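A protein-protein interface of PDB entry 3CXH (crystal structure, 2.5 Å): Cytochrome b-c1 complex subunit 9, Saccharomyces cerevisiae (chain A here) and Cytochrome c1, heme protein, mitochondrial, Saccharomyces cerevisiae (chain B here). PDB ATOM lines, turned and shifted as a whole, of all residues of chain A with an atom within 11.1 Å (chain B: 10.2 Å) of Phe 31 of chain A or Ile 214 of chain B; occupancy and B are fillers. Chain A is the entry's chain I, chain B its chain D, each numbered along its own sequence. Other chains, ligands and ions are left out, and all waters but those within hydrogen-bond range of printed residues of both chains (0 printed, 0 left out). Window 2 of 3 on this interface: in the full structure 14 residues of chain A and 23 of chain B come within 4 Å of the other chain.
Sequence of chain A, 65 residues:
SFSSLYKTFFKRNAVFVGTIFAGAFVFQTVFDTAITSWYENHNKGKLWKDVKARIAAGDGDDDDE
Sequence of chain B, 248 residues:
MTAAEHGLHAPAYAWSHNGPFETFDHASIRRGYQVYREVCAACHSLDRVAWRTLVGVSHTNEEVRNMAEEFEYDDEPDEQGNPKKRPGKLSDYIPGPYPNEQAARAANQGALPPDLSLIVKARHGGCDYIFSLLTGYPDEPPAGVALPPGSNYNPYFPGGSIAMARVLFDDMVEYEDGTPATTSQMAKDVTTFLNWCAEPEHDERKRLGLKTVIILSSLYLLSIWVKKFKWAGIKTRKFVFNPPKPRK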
ATOM      1  N   GLY A  23      24.211 -32.593  20.128  1.00  0.00           N
ATOM      2  CA  GLY A  23      23.195 -31.594  19.847  1.00  0.00           C
ATOM      3  C   GLY A  23      21.936 -31.792  20.670  1.00  0.00           C
ATOM      4  O   GLY A  23      21.244 -30.832  21.006  1.00  0.00           O
ATOM      5  N   ALA A  24      21.631 -33.048  20.986  1.00  0.00           N
ATOM      6  CA  ALA A  24      20.456 -33.375  21.789  1.00  0.00           C
ATOM      7  C   ALA A  24      20.600 -32.814  23.196  1.00  0.00           C
ATOM      8  O   ALA A  24      19.651 -32.275  23.753  1.00  0.00           O
ATOM      9  CB  ALA A  24      20.248 -34.885  21.843  1.00  0.00           C
ATOM     10  N   PHE A  25      21.801 -32.922  23.757  1.00  0.00           N
ATOM     11  CA  PHE A  25      22.059 -32.418  25.103  1.00  0.00           C
ATOM     12  C   PHE A  25      21.875 -30.905  25.171  1.00  0.00           C
ATOM     13  O   PHE A  25      21.246 -30.398  26.094  1.00  0.00           O
ATOM     14  CB  PHE A  25      23.463 -32.814  25.592  1.00  0.00           C
ATOM     15  CG  PHE A  25      23.671 -34.312  25.730  1.00  0.00           C
ATOM     16  CD1 PHE A  25      24.955 -34.835  25.888  1.00  0.00           C
ATOM     17  CD2 PHE A  25      22.591 -35.199  25.686  1.00  0.00           C
ATOM     18  CE1 PHE A  25      25.160 -36.219  25.997  1.00  0.00           C
ATOM     19  CE2 PHE A  25      22.786 -36.579  25.793  1.00  0.00           C
ATOM     20  CZ  PHE A  25      24.069 -37.090  25.949  1.00  0.00           C
ATOM     21  N   VAL A  26      22.397 -30.192  24.177  1.00  0.00           N
ATOM     22  CA  VAL A  26      22.266 -28.739  24.137  1.00  0.00           C
ATOM     23  C   VAL A  26      20.792 -28.376  23.993  1.00  0.00           C
ATOM     24  O   VAL A  26      20.254 -27.594  24.776  1.00  0.00           O
ATOM     25  CB  VAL A  26      23.061 -28.134  22.962  1.00  0.00           C
ATOM     26  CG1 VAL A  26      22.883 -26.624  22.926  1.00  0.00           C
ATOM     27  CG2 VAL A  26      24.540 -28.490  23.095  1.00  0.00           C
ATOM     28  N   PHE A  27      20.142 -28.988  23.008  1.00  0.00           N
ATOM     29  CA  PHE A  27      18.729 -28.763  22.748  1.00  0.00           C
ATOM     30  C   PHE A  27      17.868 -28.973  23.988  1.00  0.00           C
ATOM     31  O   PHE A  27      17.026 -28.137  24.311  1.00  0.00           O
ATOM     32  CB  PHE A  27      18.240 -29.693  21.634  1.00  0.00           C
ATOM     33  CG  PHE A  27      16.748 -29.671  21.439  1.00  0.00           C
ATOM     34  CD1 PHE A  27      16.162 -28.756  20.580  1.00  0.00           C
ATOM     35  CD2 PHE A  27      15.930 -30.568  22.120  1.00  0.00           C
ATOM     36  CE1 PHE A  27      14.777 -28.735  20.403  1.00  0.00           C
ATOM     37  CE2 PHE A  27      14.555 -30.552  21.950  1.00  0.00           C
ATOM     38  CZ  PHE A  27      13.975 -29.636  21.092  1.00  0.00           C
ATOM     39  N   GLN A  28      18.089 -30.082  24.682  1.00  0.00           N
ATOM     40  CA  GLN A  28      17.313 -30.409  25.870  1.00  0.00           C
ATOM     41  C   GLN A  28      17.240 -29.288  26.898  1.00  0.00           C
ATOM     42  O   GLN A  28      16.196 -29.081  27.520  1.00  0.00           O
ATOM     43  CB  GLN A  28      17.846 -31.682  26.517  1.00  0.00           C
ATOM     44  CG  GLN A  28      16.846 -32.359  27.434  1.00  0.00           C
ATOM     45  CD  GLN A  28      16.929 -33.877  27.363  1.00  0.00           C
ATOM     46  OE1 GLN A  28      16.326 -34.505  26.483  1.00  0.00           O
ATOM     47  NE2 GLN A  28      17.681 -34.475  28.290  1.00  0.00           N
ATOM     48  N   THR A  29      18.339 -28.556  27.063  1.00  0.00           N
ATOM     49  CA  THR A  29      18.394 -27.453  28.018  1.00  0.00           C
ATOM     50  C   THR A  29      17.838 -26.145  27.443  1.00  0.00           C
ATOM     51  O   THR A  29      17.049 -25.455  28.094  1.00  0.00           O
ATOM     52  CB  THR A  29      19.836 -27.226  28.536  1.00  0.00           C
ATOM     53  OG1 THR A  29      20.749 -27.262  27.435  1.00  0.00           O
ATOM     54  CG2 THR A  29      20.231 -28.305  29.531  1.00  0.00           C
ATOM     55  N   VAL A  30      18.236 -25.818  26.217  1.00  0.00           N
ATOM     56  CA  VAL A  30      17.785 -24.597  25.564  1.00  0.00           C
ATOM     57  C   VAL A  30      16.275 -24.592  25.386  1.00  0.00           C
ATOM     58  O   VAL A  30      15.601 -23.597  25.674  1.00  0.00           O
ATOM     59  CB  VAL A  30      18.478 -24.413  24.194  1.00  0.00           C
ATOM     60  CG1 VAL A  30      17.874 -23.239  23.437  1.00  0.00           C
ATOM     61  CG2 VAL A  30      19.970 -24.182  24.400  1.00  0.00           C
ATOM     62  N   PHE A  31      15.747 -25.725  24.944  1.00  0.00           N
ATOM     63  CA  PHE A  31      14.316 -25.876  24.721  1.00  0.00           C
ATOM     64  C   PHE A  31      13.515 -25.781  26.022  1.00  0.00           C
ATOM     65  O   PHE A  31      12.441 -25.181  26.047  1.00  0.00           O
ATOM     66  CB  PHE A  31      14.052 -27.212  24.017  1.00  0.00           C
ATOM     67  CG  PHE A  31      12.623 -27.425  23.619  1.00  0.00           C
ATOM     68  CD1 PHE A  31      12.059 -26.688  22.589  1.00  0.00           C
ATOM     69  CD2 PHE A  31      11.853 -28.397  24.245  1.00  0.00           C
ATOM     70  CE1 PHE A  31      10.744 -26.920  22.183  1.00  0.00           C
ATOM     71  CE2 PHE A  31      10.540 -28.634  23.846  1.00  0.00           C
ATOM     72  CZ  PHE A  31       9.985 -27.895  22.812  1.00  0.00           C
ATOM     73  N   ASP A  32      14.048 -26.341  27.104  1.00  0.00           N
ATOM     74  CA  ASP A  32      13.346 -26.314  28.381  1.00  0.00           C
ATOM     75  C   ASP A  32      13.202 -24.898  28.905  1.00  0.00           C
ATOM     76  O   ASP A  32      12.138 -24.515  29.393  1.00  0.00           O
ATOM     77  CB  ASP A  32      14.048 -27.183  29.423  1.00  0.00           C
ATOM     78  CG  ASP A  32      13.210 -27.378  30.676  1.00  0.00           C
ATOM     79  OD1 ASP A  32      12.083 -27.905  30.565  1.00  0.00           O
ATOM     80  OD2 ASP A  32      13.665 -26.988  31.770  1.00  0.00           O
ATOM     81  N   THR A  33      14.278 -24.124  28.792  1.00  0.00           N
ATOM     82  CA  THR A  33      14.292 -22.734  29.230  1.00  0.00           C
ATOM     83  C   THR A  33      13.272 -21.931  28.416  1.00  0.00           C
ATOM     84  O   THR A  33      12.448 -21.216  28.982  1.00  0.00           O
ATOM     85  CB  THR A  33      15.697 -22.112  29.040  1.00  0.00           C
ATOM     86  OG1 THR A  33      16.680 -22.939  29.683  1.00  0.00           O
ATOM     87  CG2 THR A  33      15.753 -20.706  29.638  1.00  0.00           C
ATOM     88  N   ALA A  34      13.299 -22.105  27.096  1.00  0.00           N
ATOM     89  CA  ALA A  34      12.392 -21.392  26.199  1.00  0.00           C
ATOM     90  C   ALA A  34      10.936 -21.682  26.500  1.00  0.00           C
ATOM     91  O   ALA A  34      10.109 -20.769  26.560  1.00  0.00           O
ATOM     92  CB  ALA A  34      12.696 -21.737  24.738  1.00  0.00           C
ATOM     93  N   ILE A  35      10.624 -22.960  26.677  1.00  0.00           N
ATOM     94  CA  ILE A  35       9.263 -23.368  26.955  1.00  0.00           C
ATOM     95  C   ILE A  35       8.805 -22.856  28.310  1.00  0.00           C
ATOM     96  O   ILE A  35       7.752 -22.220  28.404  1.00  0.00           O
ATOM     97  CB  ILE A  35       9.109 -24.903  26.851  1.00  0.00           C
ATOM     98  CG1 ILE A  35       9.269 -25.340  25.394  1.00  0.00           C
ATOM     99  CG2 ILE A  35       7.760 -25.359  27.394  1.00  0.00           C
ATOM    100  CD1 ILE A  35       8.285 -24.695  24.445  1.00  0.00           C
ATOM    101  N   THR A  36       9.614 -23.068  29.343  1.00  0.00           N
ATOM    102  CA  THR A  36       9.244 -22.622  30.684  1.00  0.00           C
ATOM    103  C   THR A  36       8.981 -21.117  30.740  1.00  0.00           C
ATOM    104  O   THR A  36       7.988 -20.673  31.321  1.00  0.00           O
ATOM    105  CB  THR A  36      10.304 -22.993  31.731  1.00  0.00           C
ATOM    106  OG1 THR A  36      10.539 -24.406  31.704  1.00  0.00           O
ATOM    107  CG2 THR A  36       9.820 -22.611  33.111  1.00  0.00           C
ATOM    108  N   SER A  37       9.857 -20.336  30.115  1.00  0.00           N
ATOM    109  CA  SER A  37       9.702 -18.886  30.098  1.00  0.00           C
ATOM    110  C   SER A  37       8.403 -18.480  29.421  1.00  0.00           C
ATOM    111  O   SER A  37       7.645 -17.676  29.962  1.00  0.00           O
ATOM    112  CB  SER A  37      10.885 -18.228  29.395  1.00  0.00           C
ATOM    113  OG  SER A  37      12.055 -18.388  30.170  1.00  0.00           O
ATOM    114  N   TRP A  38       8.135 -19.060  28.252  1.00  0.00           N
ATOM    115  CA  TRP A  38       6.920 -18.753  27.511  1.00  0.00           C
ATOM    116  C   TRP A  38       5.703 -19.130  28.348  1.00  0.00           C
ATOM    117  O   TRP A  38       4.785 -18.331  28.522  1.00  0.00           O
ATOM    118  CB  TRP A  38       6.888 -19.512  26.184  1.00  0.00           C
ATOM    119  CG  TRP A  38       5.732 -19.105  25.320  1.00  0.00           C
ATOM    120  CD1 TRP A  38       5.741 -18.145  24.353  1.00  0.00           C
ATOM    121  CD2 TRP A  38       4.379 -19.589  25.393  1.00  0.00           C
ATOM    122  NE1 TRP A  38       4.480 -17.987  23.827  1.00  0.00           N
ATOM    123  CE2 TRP A  38       3.625 -18.859  24.447  1.00  0.00           C
ATOM    124  CE3 TRP A  38       3.733 -20.562  26.168  1.00  0.00           C
ATOM    125  CZ2 TRP A  38       2.251 -19.071  24.253  1.00  0.00           C
ATOM    126  CZ3 TRP A  38       2.371 -20.774  25.977  1.00  0.00           C
ATOM    127  CH2 TRP A  38       1.645 -20.030  25.026  1.00  0.00           C
ATOM    128  N   TYR A  39       5.712 -20.354  28.868  1.00  0.00           N
ATOM    129  CA  TYR A  39       4.620 -20.865  29.687  1.00  0.00           C
ATOM    130  C   TYR A  39       4.364 -19.984  30.911  1.00  0.00           C
ATOM    131  O   TYR A  39       3.222 -19.617  31.181  1.00  0.00           O
ATOM    132  CB  TYR A  39       4.929 -22.306  30.117  1.00  0.00           C
ATOM    133  CG  TYR A  39       3.783 -23.026  30.788  1.00  0.00           C
ATOM    134  CD1 TYR A  39       2.667 -23.431  30.055  1.00  0.00           C
ATOM    135  CD2 TYR A  39       3.824 -23.327  32.150  1.00  0.00           C
ATOM    136  CE1 TYR A  39       1.619 -24.121  30.657  1.00  0.00           C
ATOM    137  CE2 TYR A  39       2.784 -24.016  32.761  1.00  0.00           C
ATOM    138  CZ  TYR A  39       1.685 -24.409  32.005  1.00  0.00           C
ATOM    139  OH  TYR A  39       0.650 -25.087  32.600  1.00  0.00           O
ATOM    140  N   GLU A  40       5.426 -19.651  31.643  1.00  0.00           N
ATOM    141  CA  GLU A  40       5.297 -18.812  32.839  1.00  0.00           C
ATOM    142  C   GLU A  40       4.846 -17.392  32.515  1.00  0.00           C
ATOM    143  O   GLU A  40       4.053 -16.792  33.245  1.00  0.00           O
ATOM    144  CB  GLU A  40       6.607 -18.765  33.628  1.00  0.00           C
ATOM    145  CG  GLU A  40       6.844 -19.989  34.494  1.00  0.00           C
ATOM    146  CD  GLU A  40       8.001 -19.814  35.467  1.00  0.00           C
ATOM    147  OE1 GLU A  40       8.302 -20.780  36.202  1.00  0.00           O
ATOM    148  OE2 GLU A  40       8.604 -18.716  35.508  1.00  0.00           O
ATOM    149  N   PHE B  21      -2.797 -24.069  27.333  1.00  0.00           N
ATOM    150  CA  PHE B  21      -1.679 -23.298  27.854  1.00  0.00           C
ATOM    151  C   PHE B  21      -1.910 -22.676  29.221  1.00  0.00           C
ATOM    152  O   PHE B  21      -1.013 -22.045  29.768  1.00  0.00           O
ATOM    153  CB  PHE B  21      -1.297 -22.215  26.848  1.00  0.00           C
ATOM    154  CG  PHE B  21      -1.261 -22.698  25.420  1.00  0.00           C
ATOM    155  CD1 PHE B  21      -2.046 -22.083  24.444  1.00  0.00           C
ATOM    156  CD2 PHE B  21      -0.459 -23.776  25.053  1.00  0.00           C
ATOM    157  CE1 PHE B  21      -2.034 -22.539  23.121  1.00  0.00           C
ATOM    158  CE2 PHE B  21      -0.437 -24.239  23.738  1.00  0.00           C
ATOM    159  CZ  PHE B  21      -1.227 -23.622  22.766  1.00  0.00           C
ATOM    160  N   LYS B 206       0.604 -29.819  32.100  1.00  0.00           N
ATOM    161  CA  LYS B 206       0.386 -28.971  30.943  1.00  0.00           C
ATOM    162  C   LYS B 206       1.670 -28.375  30.358  1.00  0.00           C
ATOM    163  O   LYS B 206       1.767 -28.177  29.144  1.00  0.00           O
ATOM    164  CB  LYS B 206      -0.620 -27.890  31.270  1.00  0.00           C
ATOM    165  CG  LYS B 206      -2.033 -28.395  31.354  1.00  0.00           C
ATOM    166  CD  LYS B 206      -2.968 -27.222  31.309  1.00  0.00           C
ATOM    167  CE  LYS B 206      -4.400 -27.634  31.362  1.00  0.00           C
ATOM    168  NZ  LYS B 206      -5.224 -26.412  31.465  1.00  0.00           N
ATOM    169  N   ARG B 207       2.664 -28.110  31.202  1.00  0.00           N
ATOM    170  CA  ARG B 207       3.932 -27.577  30.691  1.00  0.00           C
ATOM    171  C   ARG B 207       4.662 -28.690  29.925  1.00  0.00           C
ATOM    172  O   ARG B 207       5.169 -28.470  28.823  1.00  0.00           O
ATOM    173  CB  ARG B 207       4.827 -27.064  31.820  1.00  0.00           C
ATOM    174  CG  ARG B 207       5.993 -26.246  31.321  1.00  0.00           C
ATOM    175  CD  ARG B 207       7.076 -26.116  32.375  1.00  0.00           C
ATOM    176  NE  ARG B 207       8.228 -26.955  32.056  1.00  0.00           N
ATOM    177  CZ  ARG B 207       8.860 -27.715  32.941  1.00  0.00           C
ATOM    178  NH1 ARG B 207       9.892 -28.451  32.567  1.00  0.00           N
ATOM    179  NH2 ARG B 207       8.466 -27.729  34.204  1.00  0.00           N
ATOM    180  N   LEU B 208       4.714 -29.884  30.515  1.00  0.00           N
ATOM    181  CA  LEU B 208       5.363 -31.014  29.865  1.00  0.00           C
ATOM    182  C   LEU B 208       4.588 -31.358  28.599  1.00  0.00           C
ATOM    183  O   LEU B 208       5.175 -31.793  27.606  1.00  0.00           O
ATOM    184  CB  LEU B 208       5.450 -32.230  30.797  1.00  0.00           C
ATOM    185  CG  LEU B 208       6.316 -32.078  32.054  1.00  0.00           C
ATOM    186  CD1 LEU B 208       6.432 -33.409  32.763  1.00  0.00           C
ATOM    187  CD2 LEU B 208       7.705 -31.559  31.692  1.00  0.00           C
ATOM    188  N   GLY B 209       3.280 -31.105  28.618  1.00  0.00           N
ATOM    189  CA  GLY B 209       2.459 -31.378  27.449  1.00  0.00           C
ATOM    190  C   GLY B 209       2.883 -30.534  26.259  1.00  0.00           C
ATOM    191  O   GLY B 209       2.973 -31.024  25.134  1.00  0.00           O
ATOM    192  N   LEU B 210       3.190 -29.267  26.523  1.00  0.00           N
ATOM    193  CA  LEU B 210       3.611 -28.332  25.485  1.00  0.00           C
ATOM    194  C   LEU B 210       4.898 -28.788  24.801  1.00  0.00           C
ATOM    195  O   LEU B 210       4.976 -28.813  23.571  1.00  0.00           O
ATOM    196  CB  LEU B 210       3.802 -26.939  26.086  1.00  0.00           C
ATOM    197  CG  LEU B 210       4.070 -25.791  25.113  1.00  0.00           C
ATOM    198  CD1 LEU B 210       3.008 -25.790  24.024  1.00  0.00           C
ATOM    199  CD2 LEU B 210       4.066 -24.471  25.877  1.00  0.00           C
ATOM    200  N   LYS B 211       5.897 -29.153  25.601  1.00  0.00           N
ATOM    201  CA  LYS B 211       7.169 -29.623  25.069  1.00  0.00           C
ATOM    202  C   LYS B 211       6.939 -30.891  24.246  1.00  0.00           C
ATOM    203  O   LYS B 211       7.333 -30.977  23.084  1.00  0.00           O
ATOM    204  CB  LYS B 211       8.146 -29.960  26.208  1.00  0.00           C
ATOM    205  CG  LYS B 211       8.352 -28.879  27.260  1.00  0.00           C
ATOM    206  CD  LYS B 211       9.347 -29.333  28.328  1.00  0.00           C
ATOM    207  CE  LYS B 211      10.742 -29.567  27.744  1.00  0.00           C
ATOM    208  NZ  LYS B 211      11.728 -30.064  28.758  1.00  0.00           N
ATOM    209  N   THR B 212       6.243 -31.847  24.848  1.00  0.00           N
ATOM    210  CA  THR B 212       5.960 -33.133  24.227  1.00  0.00           C
ATOM    211  C   THR B 212       5.258 -33.041  22.897  1.00  0.00           C
ATOM    212  O   THR B 212       5.651 -33.701  21.938  1.00  0.00           O
ATOM    213  CB  THR B 212       5.125 -34.008  25.156  1.00  0.00           C
ATOM    214  OG1 THR B 212       5.773 -34.077  26.430  1.00  0.00           O
ATOM    215  CG2 THR B 212       4.981 -35.406  24.579  1.00  0.00           C
ATOM    216  N   VAL B 213       4.213 -32.229  22.833  1.00  0.00           N
ATOM    217  CA  VAL B 213       3.475 -32.083  21.591  1.00  0.00           C
ATOM    218  C   VAL B 213       4.258 -31.352  20.488  1.00  0.00           C
ATOM    219  O   VAL B 213       4.165 -31.722  19.310  1.00  0.00           O
ATOM    220  CB  VAL B 213       2.109 -31.427  21.851  1.00  0.00           C
ATOM    221  CG1 VAL B 213       1.436 -31.029  20.543  1.00  0.00           C
ATOM    222  CG2 VAL B 213       1.229 -32.405  22.619  1.00  0.00           C
ATOM    223  N   ILE B 214       5.047 -30.344  20.862  1.00  0.00           N
ATOM    224  CA  ILE B 214       5.827 -29.597  19.877  1.00  0.00           C
ATOM    225  C   ILE B 214       6.877 -30.514  19.274  1.00  0.00           C
ATOM    226  O   ILE B 214       7.011 -30.591  18.051  1.00  0.00           O
ATOM    227  CB  ILE B 214       6.505 -28.341  20.502  1.00  0.00           C
ATOM    228  CG1 ILE B 214       5.451 -27.256  20.764  1.00  0.00           C
ATOM    229  CG2 ILE B 214       7.644 -27.808  19.601  1.00  0.00           C
ATOM    230  CD1 ILE B 214       6.007 -26.017  21.478  1.00  0.00           C
ATOM    231  N   ILE B 215       7.590 -31.242  20.128  1.00  0.00           N
ATOM    232  CA  ILE B 215       8.621 -32.152  19.640  1.00  0.00           C
ATOM    233  C   ILE B 215       8.055 -33.272  18.767  1.00  0.00           C
ATOM    234  O   ILE B 215       8.558 -33.507  17.677  1.00  0.00           O
ATOM    235  CB  ILE B 215       9.479 -32.715  20.784  1.00  0.00           C
ATOM    236  CG1 ILE B 215      10.376 -33.833  20.270  1.00  0.00           C
ATOM    237  CG2 ILE B 215       8.611 -33.232  21.883  1.00  0.00           C
ATOM    238  CD1 ILE B 215      11.308 -34.367  21.328  1.00  0.00           C
ATOM    239  N   LEU B 216       6.975 -33.910  19.210  1.00  0.00           N
ATOM    240  CA  LEU B 216       6.357 -34.972  18.430  1.00  0.00           C
ATOM    241  C   LEU B 216       5.790 -34.470  17.097  1.00  0.00           C
ATOM    242  O   LEU B 216       5.919 -35.157  16.074  1.00  0.00           O
ATOM    243  CB  LEU B 216       5.288 -35.703  19.241  1.00  0.00           C
ATOM    244  CG  LEU B 216       5.848 -36.675  20.283  1.00  0.00           C
ATOM    245  CD1 LEU B 216       4.750 -37.143  21.206  1.00  0.00           C
ATOM    246  CD2 LEU B 216       6.531 -37.862  19.599  1.00  0.00           C
ATOM    247  N   SER B 217       5.154 -33.297  17.099  1.00  0.00           N
ATOM    248  CA  SER B 217       4.634 -32.733  15.850  1.00  0.00           C
ATOM    249  C   SER B 217       5.810 -32.612  14.884  1.00  0.00           C
ATOM    250  O   SER B 217       5.696 -32.968  13.706  1.00  0.00           O
ATOM    251  CB  SER B 217       4.035 -31.342  16.065  1.00  0.00           C
ATOM    252  OG  SER B 217       2.841 -31.394  16.818  1.00  0.00           O
ATOM    253  N   SER B 218       6.947 -32.145  15.399  1.00  0.00           N
ATOM    254  CA  SER B 218       8.146 -32.000  14.585  1.00  0.00           C
ATOM    255  C   SER B 218       8.654 -33.365  14.088  1.00  0.00           C
ATOM    256  O   SER B 218       8.903 -33.533  12.893  1.00  0.00           O
ATOM    257  CB  SER B 218       9.235 -31.256  15.358  1.00  0.00           C
ATOM    258  OG  SER B 218       8.734 -30.019  15.839  1.00  0.00           O
ATOM    259  N   LEU B 219       8.807 -34.334  14.989  1.00  0.00           N
ATOM    260  CA  LEU B 219       9.250 -35.675  14.587  1.00  0.00           C
ATOM    261  C   LEU B 219       8.362 -36.203  13.451  1.00  0.00           C
ATOM    262  O   LEU B 219       8.848 -36.706  12.445  1.00  0.00           O
ATOM    263  CB  LEU B 219       9.147 -36.641  15.768  1.00  0.00           C
ATOM    264  CG  LEU B 219      10.421 -37.102  16.484  1.00  0.00           C
ATOM    265  CD1 LEU B 219      11.669 -36.598  15.778  1.00  0.00           C
ATOM    266  CD2 LEU B 219      10.375 -36.677  17.938  1.00  0.00           C
ATOM    267  N   TYR B 220       7.053 -36.059  13.627  1.00  0.00           N
ATOM    268  CA  TYR B 220       6.074 -36.496  12.651  1.00  0.00           C
ATOM    269  C   TYR B 220       6.291 -35.842  11.295  1.00  0.00           C
ATOM    270  O   TYR B 220       6.338 -36.531  10.276  1.00  0.00           O
ATOM    271  CB  TYR B 220       4.674 -36.186  13.172  1.00  0.00           C
ATOM    272  CG  TYR B 220       3.560 -36.491  12.205  1.00  0.00           C
ATOM    273  CD1 TYR B 220       3.419 -37.757  11.651  1.00  0.00           C
ATOM    274  CD2 TYR B 220       2.640 -35.507  11.846  1.00  0.00           C
ATOM    275  CE1 TYR B 220       2.389 -38.038  10.760  1.00  0.00           C
ATOM    276  CE2 TYR B 220       1.609 -35.776  10.953  1.00  0.00           C
ATOM    277  CZ  TYR B 220       1.491 -37.042  10.414  1.00  0.00           C
ATOM    278  OH  TYR B 220       0.485 -37.309   9.516  1.00  0.00           O
ATOM    279  N   LEU B 221       6.419 -34.515  11.270  1.00  0.00           N
ATOM    280  CA  LEU B 221       6.639 -33.812  10.004  1.00  0.00           C
ATOM    281  C   LEU B 221       7.981 -34.231   9.402  1.00  0.00           C
ATOM    282  O   LEU B 221       8.060 -34.505   8.202  1.00  0.00           O
ATOM    283  CB  LEU B 221       6.558 -32.289  10.180  1.00  0.00           C
ATOM    284  CG  LEU B 221       5.215 -31.747  10.697  1.00  0.00           C
ATOM    285  CD1 LEU B 221       5.300 -30.241  10.890  1.00  0.00           C
ATOM    286  CD2 LEU B 221       4.072 -32.104   9.761  1.00  0.00           C
ATOM    287  N   LEU B 222       9.004 -34.353  10.246  1.00  0.00           N
ATOM    288  CA  LEU B 222      10.335 -34.771   9.792  1.00  0.00           C
ATOM    289  C   LEU B 222      10.324 -36.174   9.185  1.00  0.00           C
ATOM    290  O   LEU B 222      10.910 -36.402   8.118  1.00  0.00           O
ATOM    291  CB  LEU B 222      11.350 -34.759  10.934  1.00  0.00           C
ATOM    292  CG  LEU B 222      12.173 -33.501  11.204  1.00  0.00           C
ATOM    293  CD1 LEU B 222      12.717 -32.971   9.900  1.00  0.00           C
ATOM    294  CD2 LEU B 222      11.334 -32.467  11.873  1.00  0.00           C
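The guanidinium group of Arg 207 of chain B lies within salt-bridge range of the side-chain carboxylate of Asp 32 of chain A (3.0 Å).
NE of Arg 207 of chain B is in hydrogen-bond range of OG1 of Thr 36 of chain A, at 3.5 Å.
The side-chain carboxylate (OD1) of Asp 32 of chain A lies within salt-bridge range of the side-chain amino group (NZ) of Lys 211 of chain B, at 2.8 Å.
Lys 211 of chain B touches Phe 31 of chain A.
Phe 31 of chain A touches Ile 214 of chain B.
CG of Lys 211 of chain B touches CG2 of Ile 35 of chain A (3.6 Å).
Ile 214 of chain B touches Ile 35 of chain A (CD1 to CD1, 3.97 Å).
Trp 38 of chain A touches Phe 21 of chain B (CH2 to CG, 3.96 Å).
CE3 of Trp 38 of chain A touches CD2 of Leu 210 of chain B, 3.9 Å away.
Tyr 39 of chain A touches Phe 21 of chain B.
Tyr 39 of chain A touches Lys 206 of chain B (OH to CB, 3.4 Å).
Tyr 39 of chain A touches Arg 207 of chain B (CD2 to CG, 3.7 Å).
Of the 18 printed residues of chain B, 6 touch a printed residue of chain A.
Among the printed residues, Asp or Glu carboxylates within 4 Å of a Lys or Arg side-chain nitrogen of the other chain: Asp 32 of chain A with Arg 207 of chain B and Asp 32 of chain A with Lys 211 of chain B.
No residue of chain B comes within 4 Å of Phe 27 of chain A.
No residue of chain B comes within 4 Å of Val 30 of chain A.
Of chain B, only Lys 211 and Ile 214 come within 4 Å of Phe 31 of chain A.
Asp 32 of chain A touches just these residues of chain B: Arg 207 (3.0 Å) and Lys 211 (2.8 Å).
No residue of chain B comes within 4 Å of Ala 34 of chain A.
Of chain B, only Lys 211 (3.6 Å) and Ile 214 (3.97 Å) come within 4 Å of Ile 35 of chain A.
Ser 37 of chain A touches none of the printed residues of chain B.
Of the printed residues of chain B, Trp 38 of chain A touches Phe 21 and Leu 210.
Of the printed residues of chain B, Tyr 39 of chain A touches Phe 21, Lys 206 and Arg 207.
Printed residues of chain A within 4 Å of Phe 21 of chain B: Trp 38 and Tyr 39.
Of the printed residues of chain A, Lys 206 of chain B touches Tyr 39 (3.4 Å).
Leu 210 of chain B touches just one residue of chain A: Trp 38 (3.9 Å).
Lys 211 of chain B touches just these residues of chain A: Phe 31 (3.6 Å), Asp 32 (2.8 Å) and Ile 35 (3.6 Å).
No residue of chain A comes within 4 Å of Thr 212 of chain B.
No residue of chain A comes within 4 Å of Val 213 of chain B.
Of chain A, only Phe 31 (3.97 Å) and Ile 35 (3.97 Å) come within 4 Å of Ile 214 of chain B.
No residue of chain A comes within 4 Å of Ser 217 of chain B.
No residue of chain A comes within 4 Å of Ser 218 of chain B.
Leu 222 of chain B touches none of the printed residues of chain A.
The nearest residue of chain A that does not touch Ile 214 of chain B is Phe 27 of chain A (6.8 Å).
The backbone carbonyl oxygen (O) of Ile 214 of chain B lies within hydrogen-bond range of the side-chain hydroxyl (OG) of Ser 218 of chain B (2.9 Å).
O of Asp 32 of chain A is in hydrogen-bond range of OG1 of Thr 36 of chain A, at 2.8 Å.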
